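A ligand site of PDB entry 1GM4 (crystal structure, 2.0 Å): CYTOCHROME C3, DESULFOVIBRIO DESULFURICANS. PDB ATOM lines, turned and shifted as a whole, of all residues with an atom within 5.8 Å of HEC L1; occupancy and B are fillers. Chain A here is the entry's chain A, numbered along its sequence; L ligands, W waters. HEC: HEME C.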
ATOM      1  N   ALA A   1     -21.537  31.925  22.737  1.00  0.00           N
ATOM      2  CA  ALA A   1     -20.659  30.732  22.901  1.00  0.00           C
ATOM      3  C   ALA A   1     -20.559  30.044  21.543  1.00  0.00           C
ATOM      4  O   ALA A   1     -21.594  29.648  20.983  1.00  0.00           O
ATOM      5  CB  ALA A   1     -21.246  29.761  23.941  1.00  0.00           C
ATOM      6  N   PRO A   2     -19.335  29.959  20.980  1.00  0.00           N
ATOM      7  CA  PRO A   2     -19.164  29.309  19.673  1.00  0.00           C
ATOM      8  C   PRO A   2     -19.471  27.824  19.847  1.00  0.00           C
ATOM      9  O   PRO A   2     -19.459  27.313  20.972  1.00  0.00           O
ATOM     10  CB  PRO A   2     -17.692  29.546  19.364  1.00  0.00           C
ATOM     11  CG  PRO A   2     -17.064  29.443  20.732  1.00  0.00           C
ATOM     12  CD  PRO A   2     -18.026  30.258  21.591  1.00  0.00           C
ATOM     13  N   ALA A   3     -19.779  27.158  18.749  1.00  0.00           N
ATOM     14  CA  ALA A   3     -20.085  25.733  18.780  1.00  0.00           C
ATOM     15  C   ALA A   3     -18.861  24.928  19.179  1.00  0.00           C
ATOM     16  O   ALA A   3     -17.735  25.263  18.830  1.00  0.00           O
ATOM     17  CB  ALA A   3     -20.589  25.268  17.422  1.00  0.00           C
ATOM     18  N   VAL A   4     -19.090  23.851  19.909  1.00  0.00           N
ATOM     19  CA  VAL A   4     -18.002  22.982  20.309  1.00  0.00           C
ATOM     20  C   VAL A   4     -17.597  22.162  19.058  1.00  0.00           C
ATOM     21  O   VAL A   4     -18.473  21.759  18.262  1.00  0.00           O
ATOM     22  CB  VAL A   4     -18.471  22.063  21.464  1.00  0.00           C
ATOM     23  CG1 VAL A   4     -19.572  21.102  20.994  1.00  0.00           C
ATOM     24  CG2 VAL A   4     -17.301  21.321  22.071  1.00  0.00           C
ATOM     25  N   PRO A   5     -16.290  22.005  18.799  1.00  0.00           N
ATOM     26  CA  PRO A   5     -15.857  21.223  17.630  1.00  0.00           C
ATOM     27  C   PRO A   5     -16.462  19.805  17.675  1.00  0.00           C
ATOM     28  O   PRO A   5     -16.490  19.170  18.747  1.00  0.00           O
ATOM     29  CB  PRO A   5     -14.336  21.178  17.791  1.00  0.00           C
ATOM     30  CG  PRO A   5     -14.032  22.483  18.398  1.00  0.00           C
ATOM     31  CD  PRO A   5     -15.128  22.638  19.451  1.00  0.00           C
ATOM     32  N   VAL A   9      -9.630  18.052  17.251  1.00  0.00           N
ATOM     33  CA  VAL A   9      -8.905  19.238  16.810  1.00  0.00           C
ATOM     34  C   VAL A   9      -7.422  19.131  17.228  1.00  0.00           C
ATOM     35  O   VAL A   9      -7.088  18.439  18.193  1.00  0.00           O
ATOM     36  CB  VAL A   9      -9.515  20.553  17.381  1.00  0.00           C
ATOM     37  CG1 VAL A   9     -10.960  20.707  16.940  1.00  0.00           C
ATOM     38  CG2 VAL A   9      -9.419  20.580  18.907  1.00  0.00           C
ATOM     39  N   GLU A  10      -6.579  19.815  16.502  1.00  0.00           N
ATOM     40  CA  GLU A  10      -5.155  19.718  16.802  1.00  0.00           C
ATOM     41  C   GLU A  10      -4.721  20.614  17.963  1.00  0.00           C
ATOM     42  O   GLU A  10      -5.130  21.771  18.055  1.00  0.00           O
ATOM     43  CB  GLU A  10      -4.265  20.194  15.636  1.00  0.00           C
ATOM     44  CG  GLU A  10      -4.633  19.648  14.263  1.00  0.00           C
ATOM     45  CD  GLU A  10      -4.061  20.517  13.132  1.00  0.00           C
ATOM     46  OE1 GLU A  10      -4.480  21.735  12.986  1.00  0.00           O
ATOM     47  OE2 GLU A  10      -3.156  20.054  12.338  1.00  0.00           O
ATOM     48  N   VAL A  11      -3.917  20.042  18.803  1.00  0.00           N
ATOM     49  CA  VAL A  11      -3.289  20.748  19.916  1.00  0.00           C
ATOM     50  C   VAL A  11      -1.813  20.711  19.578  1.00  0.00           C
ATOM     51  O   VAL A  11      -1.106  19.756  19.918  1.00  0.00           O
ATOM     52  CB  VAL A  11      -3.580  20.077  21.272  1.00  0.00           C
ATOM     53  CG1 VAL A  11      -2.986  20.865  22.445  1.00  0.00           C
ATOM     54  CG2 VAL A  11      -5.067  19.947  21.583  1.00  0.00           C
ATOM     55  N   LYS A  12      -1.386  21.747  18.887  1.00  0.00           N
ATOM     56  CA  LYS A  12       0.000  21.875  18.408  1.00  0.00           C
ATOM     57  C   LYS A  12       0.928  22.345  19.533  1.00  0.00           C
ATOM     58  O   LYS A  12       0.883  23.506  19.961  1.00  0.00           O
ATOM     59  CB  LYS A  12       0.060  22.879  17.264  1.00  0.00           C
ATOM     60  CG  LYS A  12      -0.627  22.364  15.986  1.00  0.00           C
ATOM     61  CD  LYS A  12      -0.518  23.363  14.832  1.00  0.00           C
ATOM     62  CE  LYS A  12      -0.914  22.768  13.479  1.00  0.00           C
ATOM     63  NZ  LYS A  12      -0.502  23.614  12.344  1.00  0.00           N
ATOM     64  N   PHE A  20      -7.303  16.400  20.023  1.00  0.00           N
ATOM     65  CA  PHE A  20      -8.179  16.513  21.184  1.00  0.00           C
ATOM     66  C   PHE A  20      -9.655  16.260  20.814  1.00  0.00           C
ATOM     67  O   PHE A  20     -10.234  17.003  20.018  1.00  0.00           O
ATOM     68  CB  PHE A  20      -8.013  17.887  21.846  1.00  0.00           C
ATOM     69  CG  PHE A  20      -8.993  18.130  22.978  1.00  0.00           C
ATOM     70  CD1 PHE A  20      -8.727  17.648  24.254  1.00  0.00           C
ATOM     71  CD2 PHE A  20     -10.212  18.765  22.731  1.00  0.00           C
ATOM     72  CE1 PHE A  20      -9.679  17.770  25.274  1.00  0.00           C
ATOM     73  CE2 PHE A  20     -11.156  18.890  23.740  1.00  0.00           C
ATOM     74  CZ  PHE A  20     -10.897  18.392  25.007  1.00  0.00           C
ATOM     75  N   HIS A  22     -13.505  16.402  21.746  1.00  0.00           N
ATOM     76  CA  HIS A  22     -14.442  17.029  22.668  1.00  0.00           C
ATOM     77  C   HIS A  22     -15.519  16.080  23.201  1.00  0.00           C
ATOM     78  O   HIS A  22     -15.893  16.159  24.360  1.00  0.00           O
ATOM     79  CB  HIS A  22     -15.131  18.229  21.992  1.00  0.00           C
ATOM     80  CG  HIS A  22     -14.376  19.514  22.113  1.00  0.00           C
ATOM     81  ND1 HIS A  22     -13.395  19.921  21.240  1.00  0.00           N
ATOM     82  CD2 HIS A  22     -14.473  20.513  23.037  1.00  0.00           C
ATOM     83  CE1 HIS A  22     -12.950  21.118  21.642  1.00  0.00           C
ATOM     84  NE2 HIS A  22     -13.576  21.523  22.731  1.00  0.00           N
ATOM     85  N   HIS A  25     -15.442  14.513  26.500  1.00  0.00           N
ATOM     86  CA  HIS A  25     -15.420  15.527  27.536  1.00  0.00           C
ATOM     87  C   HIS A  25     -16.757  16.246  27.681  1.00  0.00           C
ATOM     88  O   HIS A  25     -16.835  17.260  28.357  1.00  0.00           O
ATOM     89  CB  HIS A  25     -14.302  16.555  27.257  1.00  0.00           C
ATOM     90  CG  HIS A  25     -12.940  15.962  27.218  1.00  0.00           C
ATOM     91  ND1 HIS A  25     -12.369  15.408  26.085  1.00  0.00           N
ATOM     92  CD2 HIS A  25     -12.044  15.745  28.212  1.00  0.00           C
ATOM     93  CE1 HIS A  25     -11.195  14.869  26.416  1.00  0.00           C
ATOM     94  NE2 HIS A  25     -10.945  15.044  27.702  1.00  0.00           N
ATOM     95  N   VAL A  28     -17.787  17.660  31.039  1.00  0.00           N
ATOM     96  CA  VAL A  28     -16.807  18.512  31.722  1.00  0.00           C
ATOM     97  C   VAL A  28     -17.288  19.905  31.315  1.00  0.00           C
ATOM     98  O   VAL A  28     -17.602  20.119  30.144  1.00  0.00           O
ATOM     99  CB  VAL A  28     -15.332  18.276  31.213  1.00  0.00           C
ATOM    100  CG1 VAL A  28     -14.365  19.205  31.925  1.00  0.00           C
ATOM    101  CG2 VAL A  28     -14.909  16.837  31.451  1.00  0.00           C
ATOM    102  N   GLU A  29     -17.450  20.828  32.269  1.00  0.00           N
ATOM    103  CA  GLU A  29     -17.878  22.176  31.958  1.00  0.00           C
ATOM    104  C   GLU A  29     -16.861  22.810  31.013  1.00  0.00           C
ATOM    105  O   GLU A  29     -15.657  22.662  31.215  1.00  0.00           O
ATOM    106  CB  GLU A  29     -17.977  23.037  33.215  1.00  0.00           C
ATOM    107  CG  GLU A  29     -19.080  22.605  34.163  1.00  0.00           C
ATOM    108  CD  GLU A  29     -19.156  23.469  35.418  1.00  0.00           C
ATOM    109  OE1 GLU A  29     -18.313  24.373  35.621  1.00  0.00           O
ATOM    110  OE2 GLU A  29     -20.093  23.236  36.220  1.00  0.00           O
ATOM    111  N   CYS A  30     -17.358  23.514  30.008  1.00  0.00           N
ATOM    112  CA  CYS A  30     -16.489  24.160  29.034  1.00  0.00           C
ATOM    113  C   CYS A  30     -15.436  24.993  29.753  1.00  0.00           C
ATOM    114  O   CYS A  30     -14.243  24.912  29.417  1.00  0.00           O
ATOM    115  CB  CYS A  30     -17.299  25.116  28.126  1.00  0.00           C
ATOM    116  SG  CYS A  30     -18.667  24.391  27.224  1.00  0.00           S
ATOM    117  N   THR A  32     -14.014  24.697  32.572  1.00  0.00           N
ATOM    118  CA  THR A  32     -12.928  23.989  33.229  1.00  0.00           C
ATOM    119  C   THR A  32     -11.670  24.156  32.369  1.00  0.00           C
ATOM    120  O   THR A  32     -10.581  24.399  32.889  1.00  0.00           O
ATOM    121  CB  THR A  32     -13.248  22.511  33.360  1.00  0.00           C
ATOM    122  OG1 THR A  32     -14.444  22.349  34.141  1.00  0.00           O
ATOM    123  CG2 THR A  32     -12.103  21.772  34.022  1.00  0.00           C
ATOM    124  N   CYS A  33     -11.829  24.031  31.054  1.00  0.00           N
ATOM    125  CA  CYS A  33     -10.697  24.131  30.132  1.00  0.00           C
ATOM    126  C   CYS A  33     -10.583  25.526  29.550  1.00  0.00           C
ATOM    127  O   CYS A  33      -9.512  26.129  29.635  1.00  0.00           O
ATOM    128  CB  CYS A  33     -10.821  23.086  29.041  1.00  0.00           C
ATOM    129  SG  CYS A  33     -11.057  21.440  29.716  1.00  0.00           S
ATOM    130  N   HIS A  34     -11.665  26.037  28.966  1.00  0.00           N
ATOM    131  CA  HIS A  34     -11.685  27.389  28.412  1.00  0.00           C
ATOM    132  C   HIS A  34     -12.061  28.295  29.583  1.00  0.00           C
ATOM    133  O   HIS A  34     -13.212  28.728  29.701  1.00  0.00           O
ATOM    134  CB  HIS A  34     -12.741  27.505  27.314  1.00  0.00           C
ATOM    135  CG  HIS A  34     -12.515  26.562  26.177  1.00  0.00           C
ATOM    136  ND1 HIS A  34     -11.460  26.649  25.295  1.00  0.00           N
ATOM    137  CD2 HIS A  34     -13.222  25.467  25.788  1.00  0.00           C
ATOM    138  CE1 HIS A  34     -11.558  25.638  24.418  1.00  0.00           C
ATOM    139  NE2 HIS A  34     -12.610  24.882  24.676  1.00  0.00           N
ATOM    140  N   TYR A  43     -12.590  31.413  24.155  1.00  0.00           N
ATOM    141  CA  TYR A  43     -12.516  30.097  23.544  1.00  0.00           C
ATOM    142  C   TYR A  43     -11.335  30.079  22.570  1.00  0.00           C
ATOM    143  O   TYR A  43     -11.271  29.236  21.685  1.00  0.00           O
ATOM    144  CB  TYR A  43     -13.828  29.782  22.838  1.00  0.00           C
ATOM    145  CG  TYR A  43     -14.948  29.544  23.811  1.00  0.00           C
ATOM    146  CD1 TYR A  43     -15.772  30.596  24.213  1.00  0.00           C
ATOM    147  CD2 TYR A  43     -15.167  28.279  24.364  1.00  0.00           C
ATOM    148  CE1 TYR A  43     -16.787  30.377  25.158  1.00  0.00           C
ATOM    149  CE2 TYR A  43     -16.173  28.057  25.306  1.00  0.00           C
ATOM    150  CZ  TYR A  43     -16.979  29.110  25.693  1.00  0.00           C
ATOM    151  OH  TYR A  43     -17.970  28.907  26.633  1.00  0.00           O
ATOM    152  N   ALA A  44     -10.426  31.022  22.741  1.00  0.00           N
ATOM    153  CA  ALA A  44      -9.252  31.135  21.869  1.00  0.00           C
ATOM    154  C   ALA A  44      -8.353  29.933  22.134  1.00  0.00           C
ATOM    155  O   ALA A  44      -8.444  29.322  23.195  1.00  0.00           O
ATOM    156  CB  ALA A  44      -8.493  32.444  22.177  1.00  0.00           C
ATOM    157  N   LYS A  45      -7.465  29.649  21.184  1.00  0.00           N
ATOM    158  CA  LYS A  45      -6.561  28.515  21.312  1.00  0.00           C
ATOM    159  C   LYS A  45      -5.664  28.698  22.540  1.00  0.00           C
ATOM    160  O   LYS A  45      -5.202  29.807  22.806  1.00  0.00           O
ATOM    161  CB  LYS A  45      -5.745  28.344  20.022  1.00  0.00           C
ATOM    162  CG  LYS A  45      -6.617  28.052  18.790  1.00  0.00           C
ATOM    163  CD  LYS A  45      -5.841  27.832  17.486  1.00  0.00           C
ATOM    164  CE  LYS A  45      -6.809  27.601  16.310  1.00  0.00           C
ATOM    165  NZ  LYS A  45      -6.138  27.587  14.979  1.00  0.00           N
ATOM    166  N   CYS A  46      -5.440  27.624  23.287  1.00  0.00           N
ATOM    167  CA  CYS A  46      -4.626  27.709  24.511  1.00  0.00           C
ATOM    168  C   CYS A  46      -3.267  28.332  24.236  1.00  0.00           C
ATOM    169  O   CYS A  46      -2.717  29.031  25.088  1.00  0.00           O
ATOM    170  CB  CYS A  46      -4.406  26.329  25.100  1.00  0.00           C
ATOM    171  SG  CYS A  46      -5.939  25.373  25.187  1.00  0.00           S
ATOM    172  N   GLY A  47      -2.712  28.033  23.047  1.00  0.00           N
ATOM    173  CA  GLY A  47      -1.421  28.588  22.688  1.00  0.00           C
ATOM    174  C   GLY A  47      -1.432  29.980  22.062  1.00  0.00           C
ATOM    175  O   GLY A  47      -0.416  30.422  21.560  1.00  0.00           O
ATOM    176  N   LEU A  64       2.745  25.918  27.313  1.00  0.00           N
ATOM    177  CA  LEU A  64       1.612  25.088  26.901  1.00  0.00           C
ATOM    178  C   LEU A  64       1.804  23.658  27.448  1.00  0.00           C
ATOM    179  O   LEU A  64       0.837  22.990  27.826  1.00  0.00           O
ATOM    180  CB  LEU A  64       1.475  25.031  25.373  1.00  0.00           C
ATOM    181  CG  LEU A  64       0.233  24.303  24.815  1.00  0.00           C
ATOM    182  CD1 LEU A  64      -1.035  24.909  25.384  1.00  0.00           C
ATOM    183  CD2 LEU A  64       0.199  24.332  23.294  1.00  0.00           C
HETATM  184 FE   HEC L   1     -12.990  23.180  23.702  1.00  0.00          FE
HETATM  185  CHA HEC L   1     -10.867  23.802  21.167  1.00  0.00           C
HETATM  186  CHB HEC L   1     -15.327  25.112  22.266  1.00  0.00           C
HETATM  187  CHC HEC L   1     -15.158  22.236  26.137  1.00  0.00           C
HETATM  188  CHD HEC L   1     -10.445  21.762  25.479  1.00  0.00           C
HETATM  189  NA  HEC L   1     -13.053  24.297  22.071  1.00  0.00           N
HETATM  190  C1A HEC L   1     -12.094  24.455  21.105  1.00  0.00           C
HETATM  191  C2A HEC L   1     -12.529  25.423  20.074  1.00  0.00           C
HETATM  192  C3A HEC L   1     -13.786  25.754  20.443  1.00  0.00           C
HETATM  193  C4A HEC L   1     -14.104  25.050  21.646  1.00  0.00           C
HETATM  194  CMA HEC L   1     -14.750  26.725  19.776  1.00  0.00           C
HETATM  195  CAA HEC L   1     -11.886  25.804  18.735  1.00  0.00           C
HETATM  196  CBA HEC L   1     -10.583  26.581  18.623  1.00  0.00           C
HETATM  197  CGA HEC L   1      -9.333  25.746  18.863  1.00  0.00           C
HETATM  198  O1A HEC L   1      -8.630  26.043  19.845  1.00  0.00           O
HETATM  199  O2A HEC L   1      -9.062  24.823  18.074  1.00  0.00           O
HETATM  200  NB  HEC L   1     -14.859  23.573  24.111  1.00  0.00           N
HETATM  201  C1B HEC L   1     -15.696  24.422  23.402  1.00  0.00           C
HETATM  202  C2B HEC L   1     -16.975  24.505  24.033  1.00  0.00           C
HETATM  203  C3B HEC L   1     -16.977  23.650  25.134  1.00  0.00           C
HETATM  204  C4B HEC L   1     -15.621  23.118  25.186  1.00  0.00           C
HETATM  205  CMB HEC L   1     -18.065  25.510  23.615  1.00  0.00           C
HETATM  206  CAB HEC L   1     -18.081  23.264  25.944  1.00  0.00           C
HETATM  207  CBB HEC L   1     -19.339  22.693  25.410  1.00  0.00           C
HETATM  208  NC  HEC L   1     -12.845  22.048  25.397  1.00  0.00           N
HETATM  209  C1C HEC L   1     -13.872  21.708  26.238  1.00  0.00           C
HETATM  210  C2C HEC L   1     -13.414  20.979  27.440  1.00  0.00           C
HETATM  211  C3C HEC L   1     -12.038  20.910  27.315  1.00  0.00           C
HETATM  212  C4C HEC L   1     -11.713  21.590  26.021  1.00  0.00           C
HETATM  213  CMC HEC L   1     -14.321  20.458  28.590  1.00  0.00           C
HETATM  214  CAC HEC L   1     -11.135  20.357  28.275  1.00  0.00           C
HETATM  215  CBC HEC L   1     -11.238  18.975  28.682  1.00  0.00           C
HETATM  216  ND  HEC L   1     -11.059  22.864  23.386  1.00  0.00           N
HETATM  217  C1D HEC L   1     -10.133  22.293  24.233  1.00  0.00           C
HETATM  218  C2D HEC L   1      -8.838  22.217  23.580  1.00  0.00           C
HETATM  219  C3D HEC L   1      -8.950  22.790  22.366  1.00  0.00           C
HETATM  220  C4D HEC L   1     -10.343  23.136  22.254  1.00  0.00           C
HETATM  221  CMD HEC L   1      -7.552  21.642  24.174  1.00  0.00           C
HETATM  222  CAD HEC L   1      -7.824  23.188  21.415  1.00  0.00           C
HETATM  223  CBD HEC L   1      -7.014  24.408  21.849  1.00  0.00           C
HETATM  224  CGD HEC L   1      -5.794  24.653  20.975  1.00  0.00           C
HETATM  225  O1D HEC L   1      -5.760  24.180  19.834  1.00  0.00           O
HETATM  226  O2D HEC L   1      -4.844  25.331  21.447  1.00  0.00           O
HETATM  227 FE   HEC L   2      -9.557  14.020  28.730  1.00  0.00          FE
HETATM  228  CHA HEC L   2     -10.961  11.164  27.608  1.00  0.00           C
HETATM  229  CHB HEC L   2      -7.377  14.073  26.007  1.00  0.00           C
HETATM  230  CHC HEC L   2      -8.415  17.138  29.644  1.00  0.00           C
HETATM  231  CHD HEC L   2     -11.670  14.064  31.448  1.00  0.00           C
HETATM  232  NA  HEC L   2      -9.253  12.863  27.157  1.00  0.00           N
HETATM  233  C1A HEC L   2      -9.933  11.700  26.838  1.00  0.00           C
HETATM  234  C2A HEC L   2      -9.328  11.036  25.735  1.00  0.00           C
HETATM  235  C3A HEC L   2      -8.337  11.844  25.253  1.00  0.00           C
HETATM  236  C4A HEC L   2      -8.271  12.998  26.147  1.00  0.00           C
HETATM  237  CMA HEC L   2      -7.439  11.614  24.058  1.00  0.00           C
HETATM  238  CAA HEC L   2      -9.571   9.585  25.325  1.00  0.00           C
HETATM  239  CBA HEC L   2     -10.604   9.604  24.243  1.00  0.00           C
HETATM  240  CGA HEC L   2     -10.752   8.275  23.535  1.00  0.00           C
HETATM  241  O1A HEC L   2      -9.747   7.778  22.970  1.00  0.00           O
HETATM  242  O2A HEC L   2     -11.871   7.735  23.549  1.00  0.00           O
HETATM  243  NB  HEC L   2      -8.175  15.319  27.985  1.00  0.00           N
HETATM  244  C1B HEC L   2      -7.353  15.178  26.850  1.00  0.00           C
HETATM  245  C2B HEC L   2      -6.517  16.328  26.672  1.00  0.00           C
HETATM  246  C3B HEC L   2      -6.840  17.221  27.656  1.00  0.00           C
HETATM  247  C4B HEC L   2      -7.870  16.585  28.467  1.00  0.00           C
HETATM  248  CMB HEC L   2      -5.464  16.517  25.603  1.00  0.00           C
HETATM  249  CAB HEC L   2      -6.311  18.519  27.870  1.00  0.00           C
HETATM  250  CBB HEC L   2      -6.626  19.703  26.991  1.00  0.00           C
HETATM  251  NC  HEC L   2      -9.966  15.314  30.242  1.00  0.00           N
HETATM  252  C1C HEC L   2      -9.408  16.561  30.454  1.00  0.00           C
HETATM  253  C2C HEC L   2      -9.981  17.184  31.621  1.00  0.00           C
HETATM  254  C3C HEC L   2     -10.863  16.261  32.228  1.00  0.00           C
HETATM  255  C4C HEC L   2     -10.857  15.143  31.323  1.00  0.00           C
HETATM  256  CMC HEC L   2      -9.573  18.604  32.059  1.00  0.00           C
HETATM  257  CAC HEC L   2     -11.495  16.228  33.484  1.00  0.00           C
HETATM  258  CBC HEC L   2     -12.130  17.401  34.060  1.00  0.00           C
HETATM  259  ND  HEC L   2     -10.907  12.822  29.429  1.00  0.00           N
HETATM  260  C1D HEC L   2     -11.730  13.006  30.557  1.00  0.00           C
HETATM  261  C2D HEC L   2     -12.730  11.979  30.637  1.00  0.00           C
HETATM  262  C3D HEC L   2     -12.483  11.167  29.622  1.00  0.00           C
HETATM  263  C4D HEC L   2     -11.378  11.666  28.852  1.00  0.00           C
HETATM  264  CMD HEC L   2     -13.924  11.955  31.607  1.00  0.00           C
HETATM  265  CAD HEC L   2     -13.310   9.936  29.341  1.00  0.00           C
HETATM  266  CBD HEC L   2     -12.800   8.699  30.032  1.00  0.00           C
HETATM  267  CGD HEC L   2     -13.769   7.538  29.954  1.00  0.00           C
HETATM  268  O1D HEC L   2     -13.883   6.923  28.873  1.00  0.00           O
HETATM  269  O2D HEC L   2     -14.417   7.249  30.979  1.00  0.00           O
HETATM  270 FE   HEC L   3      -5.046  29.446  30.465  1.00  0.00          FE
HETATM  271  CHA HEC L   3      -3.912  29.961  33.562  1.00  0.00           C
HETATM  272  CHB HEC L   3      -5.134  26.115  30.852  1.00  0.00           C
HETATM  273  CHC HEC L   3      -6.631  29.061  27.379  1.00  0.00           C
HETATM  274  CHD HEC L   3      -4.602  32.737  29.741  1.00  0.00           C
HETATM  275  NA  HEC L   3      -4.640  28.294  31.948  1.00  0.00           N
HETATM  276  C1A HEC L   3      -4.145  28.640  33.178  1.00  0.00           C
HETATM  277  C2A HEC L   3      -3.863  27.453  33.961  1.00  0.00           C
HETATM  278  C3A HEC L   3      -4.245  26.375  33.229  1.00  0.00           C
HETATM  279  C4A HEC L   3      -4.726  26.905  31.957  1.00  0.00           C
HETATM  280  CMA HEC L   3      -4.237  24.909  33.647  1.00  0.00           C
HETATM  281  CAA HEC L   3      -3.197  27.429  35.316  1.00  0.00           C
HETATM  282  CBA HEC L   3      -1.714  27.678  35.123  1.00  0.00           C
HETATM  283  CGA HEC L   3      -0.949  27.927  36.428  1.00  0.00           C
HETATM  284  O1A HEC L   3      -1.412  27.542  37.529  1.00  0.00           O
HETATM  285  O2A HEC L   3       0.141  28.521  36.346  1.00  0.00           O
HETATM  286  NB  HEC L   3      -5.716  27.912  29.273  1.00  0.00           N
HETATM  287  C1B HEC L   3      -5.539  26.577  29.571  1.00  0.00           C
HETATM  288  C2B HEC L   3      -5.921  25.729  28.458  1.00  0.00           C
HETATM  289  C3B HEC L   3      -6.497  26.533  27.496  1.00  0.00           C
HETATM  290  C4B HEC L   3      -6.352  27.901  28.036  1.00  0.00           C
HETATM  291  CMB HEC L   3      -5.697  24.209  28.526  1.00  0.00           C
HETATM  292  CAB HEC L   3      -7.107  26.176  26.289  1.00  0.00           C
HETATM  293  CBB HEC L   3      -8.329  25.384  26.135  1.00  0.00           C
HETATM  294  NC  HEC L   3      -5.534  30.668  28.909  1.00  0.00           N
HETATM  295  C1C HEC L   3      -6.228  30.353  27.742  1.00  0.00           C
HETATM  296  C2C HEC L   3      -6.312  31.502  26.866  1.00  0.00           C
HETATM  297  C3C HEC L   3      -5.601  32.490  27.450  1.00  0.00           C
HETATM  298  C4C HEC L   3      -5.195  31.998  28.759  1.00  0.00           C
HETATM  299  CMC HEC L   3      -7.143  31.616  25.597  1.00  0.00           C
HETATM  300  CAC HEC L   3      -5.238  33.727  26.893  1.00  0.00           C
HETATM  301  CBC HEC L   3      -6.229  34.778  26.637  1.00  0.00           C
HETATM  302  ND  HEC L   3      -4.347  31.032  31.444  1.00  0.00           N
HETATM  303  C1D HEC L   3      -4.206  32.322  30.994  1.00  0.00           C
HETATM  304  C2D HEC L   3      -3.791  33.214  32.070  1.00  0.00           C
HETATM  305  C3D HEC L   3      -3.698  32.443  33.189  1.00  0.00           C
HETATM  306  C4D HEC L   3      -3.997  31.087  32.767  1.00  0.00           C
HETATM  307  CMD HEC L   3      -3.388  34.682  31.871  1.00  0.00           C
HETATM  308  CAD HEC L   3      -3.400  32.860  34.620  1.00  0.00           C
HETATM  309  CBD HEC L   3      -4.607  33.433  35.364  1.00  0.00           C
HETATM  310  CGD HEC L   3      -5.762  32.447  35.434  1.00  0.00           C
HETATM  311  O1D HEC L   3      -6.834  32.749  34.854  1.00  0.00           O
HETATM  312  O2D HEC L   3      -5.597  31.384  36.064  1.00  0.00           O
HETATM  313  O   HOH W   1     -17.443  20.048  27.368  1.00  0.00           O
HETATM  314  O   HOH W   2      -9.661  26.961  22.525  1.00  0.00           O
HETATM  315  O   HOH W   3     -20.109  19.873  27.087  1.00  0.00           O
HETATM  316  O   HOH W   4      -6.705  23.631  16.709  1.00  0.00           O
HETATM  317  O   HOH W   5      -3.241  24.154  18.831  1.00  0.00           O
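The side-chain sulfur of Cys 30 is bonded to a carbon (CAB) of HEC L1.
A carbon (CAC) of HEC L1 is covalently linked to the side-chain sulfur of Cys 33, 1.8 Å away.
An iron atom (FE) of HEC L1 is bound by a ring nitrogen (NE2) of His 34, at 2.0 Å.
An iron atom (FE) of HEC L1 is bound by a ring nitrogen (NE2) of His 22 (2.0 Å).
The backbone NH (N) of Cys 46 is in hydrogen-bond range of an oxygen (O2D) of HEC L1, at 3.0 Å.
The backbone carbonyl oxygen of Glu 10 lies close to an oxygen (O1D) of HEC L1 (3.1 Å).
An iron atom (FE) of HEC L2 is bound by a ring nitrogen (NE2) of His 25, at 2.0 Å.
The side-chain sulfur (SG) of Cys 46 is bonded to a carbon (CAB) of HEC L3, 1.8 Å away.
The backbone NH (N) of Phe 20 is in hydrogen-bond range of the backbone carbonyl oxygen (O) of Val 9 (2.7 Å).
The backbone carbonyl oxygen (O) of Glu 29 is in hydrogen-bond range of the side-chain hydroxyl (OG1) of Thr 32, at 3.2 Å.
Merely in contact with HEC L1: Lys 45 (3.0 Å), His 25 (3.4 Å), Pro 5 (3.4 Å), Phe 20 (3.4 Å), Ala 3 (3.5 Å), Pro 2 (3.5 Å), Val 28 (3.6 Å), Tyr 43 (3.6 Å), Glu 29 (3.7 Å), Val 4 (3.7 Å), Gly 47 (3.8 Å), Val 9 (3.95 Å) and Val 11 (3.97 Å).
Hydrophobic or aromatic side chains that line HEC L1: Pro 2, Val 4, Pro 5, Val 9, Val 11, Phe 20, His 22, His 25, Val 28, His 34 and Tyr 43.
Water W5 lies within hydrogen-bond range of an oxygen (O1D) of HEC L1 (2.7 Å), the backbone NH (N) of Lys 12 (3.0 Å) and the backbone carbonyl oxygen (O) of Glu 10 (3.1 Å).
Water W4 bridges O of Glu 10 (2.8 Å) and O2A of HEC L1 (3.0 Å).
Water W2 lies within hydrogen-bond range of the backbone carbonyl oxygen (O) of Ala 44, the backbone carbonyl oxygen (O) of Tyr 43, an oxygen (O1A) of HEC L1 and a ring nitrogen (ND1) of His 34.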
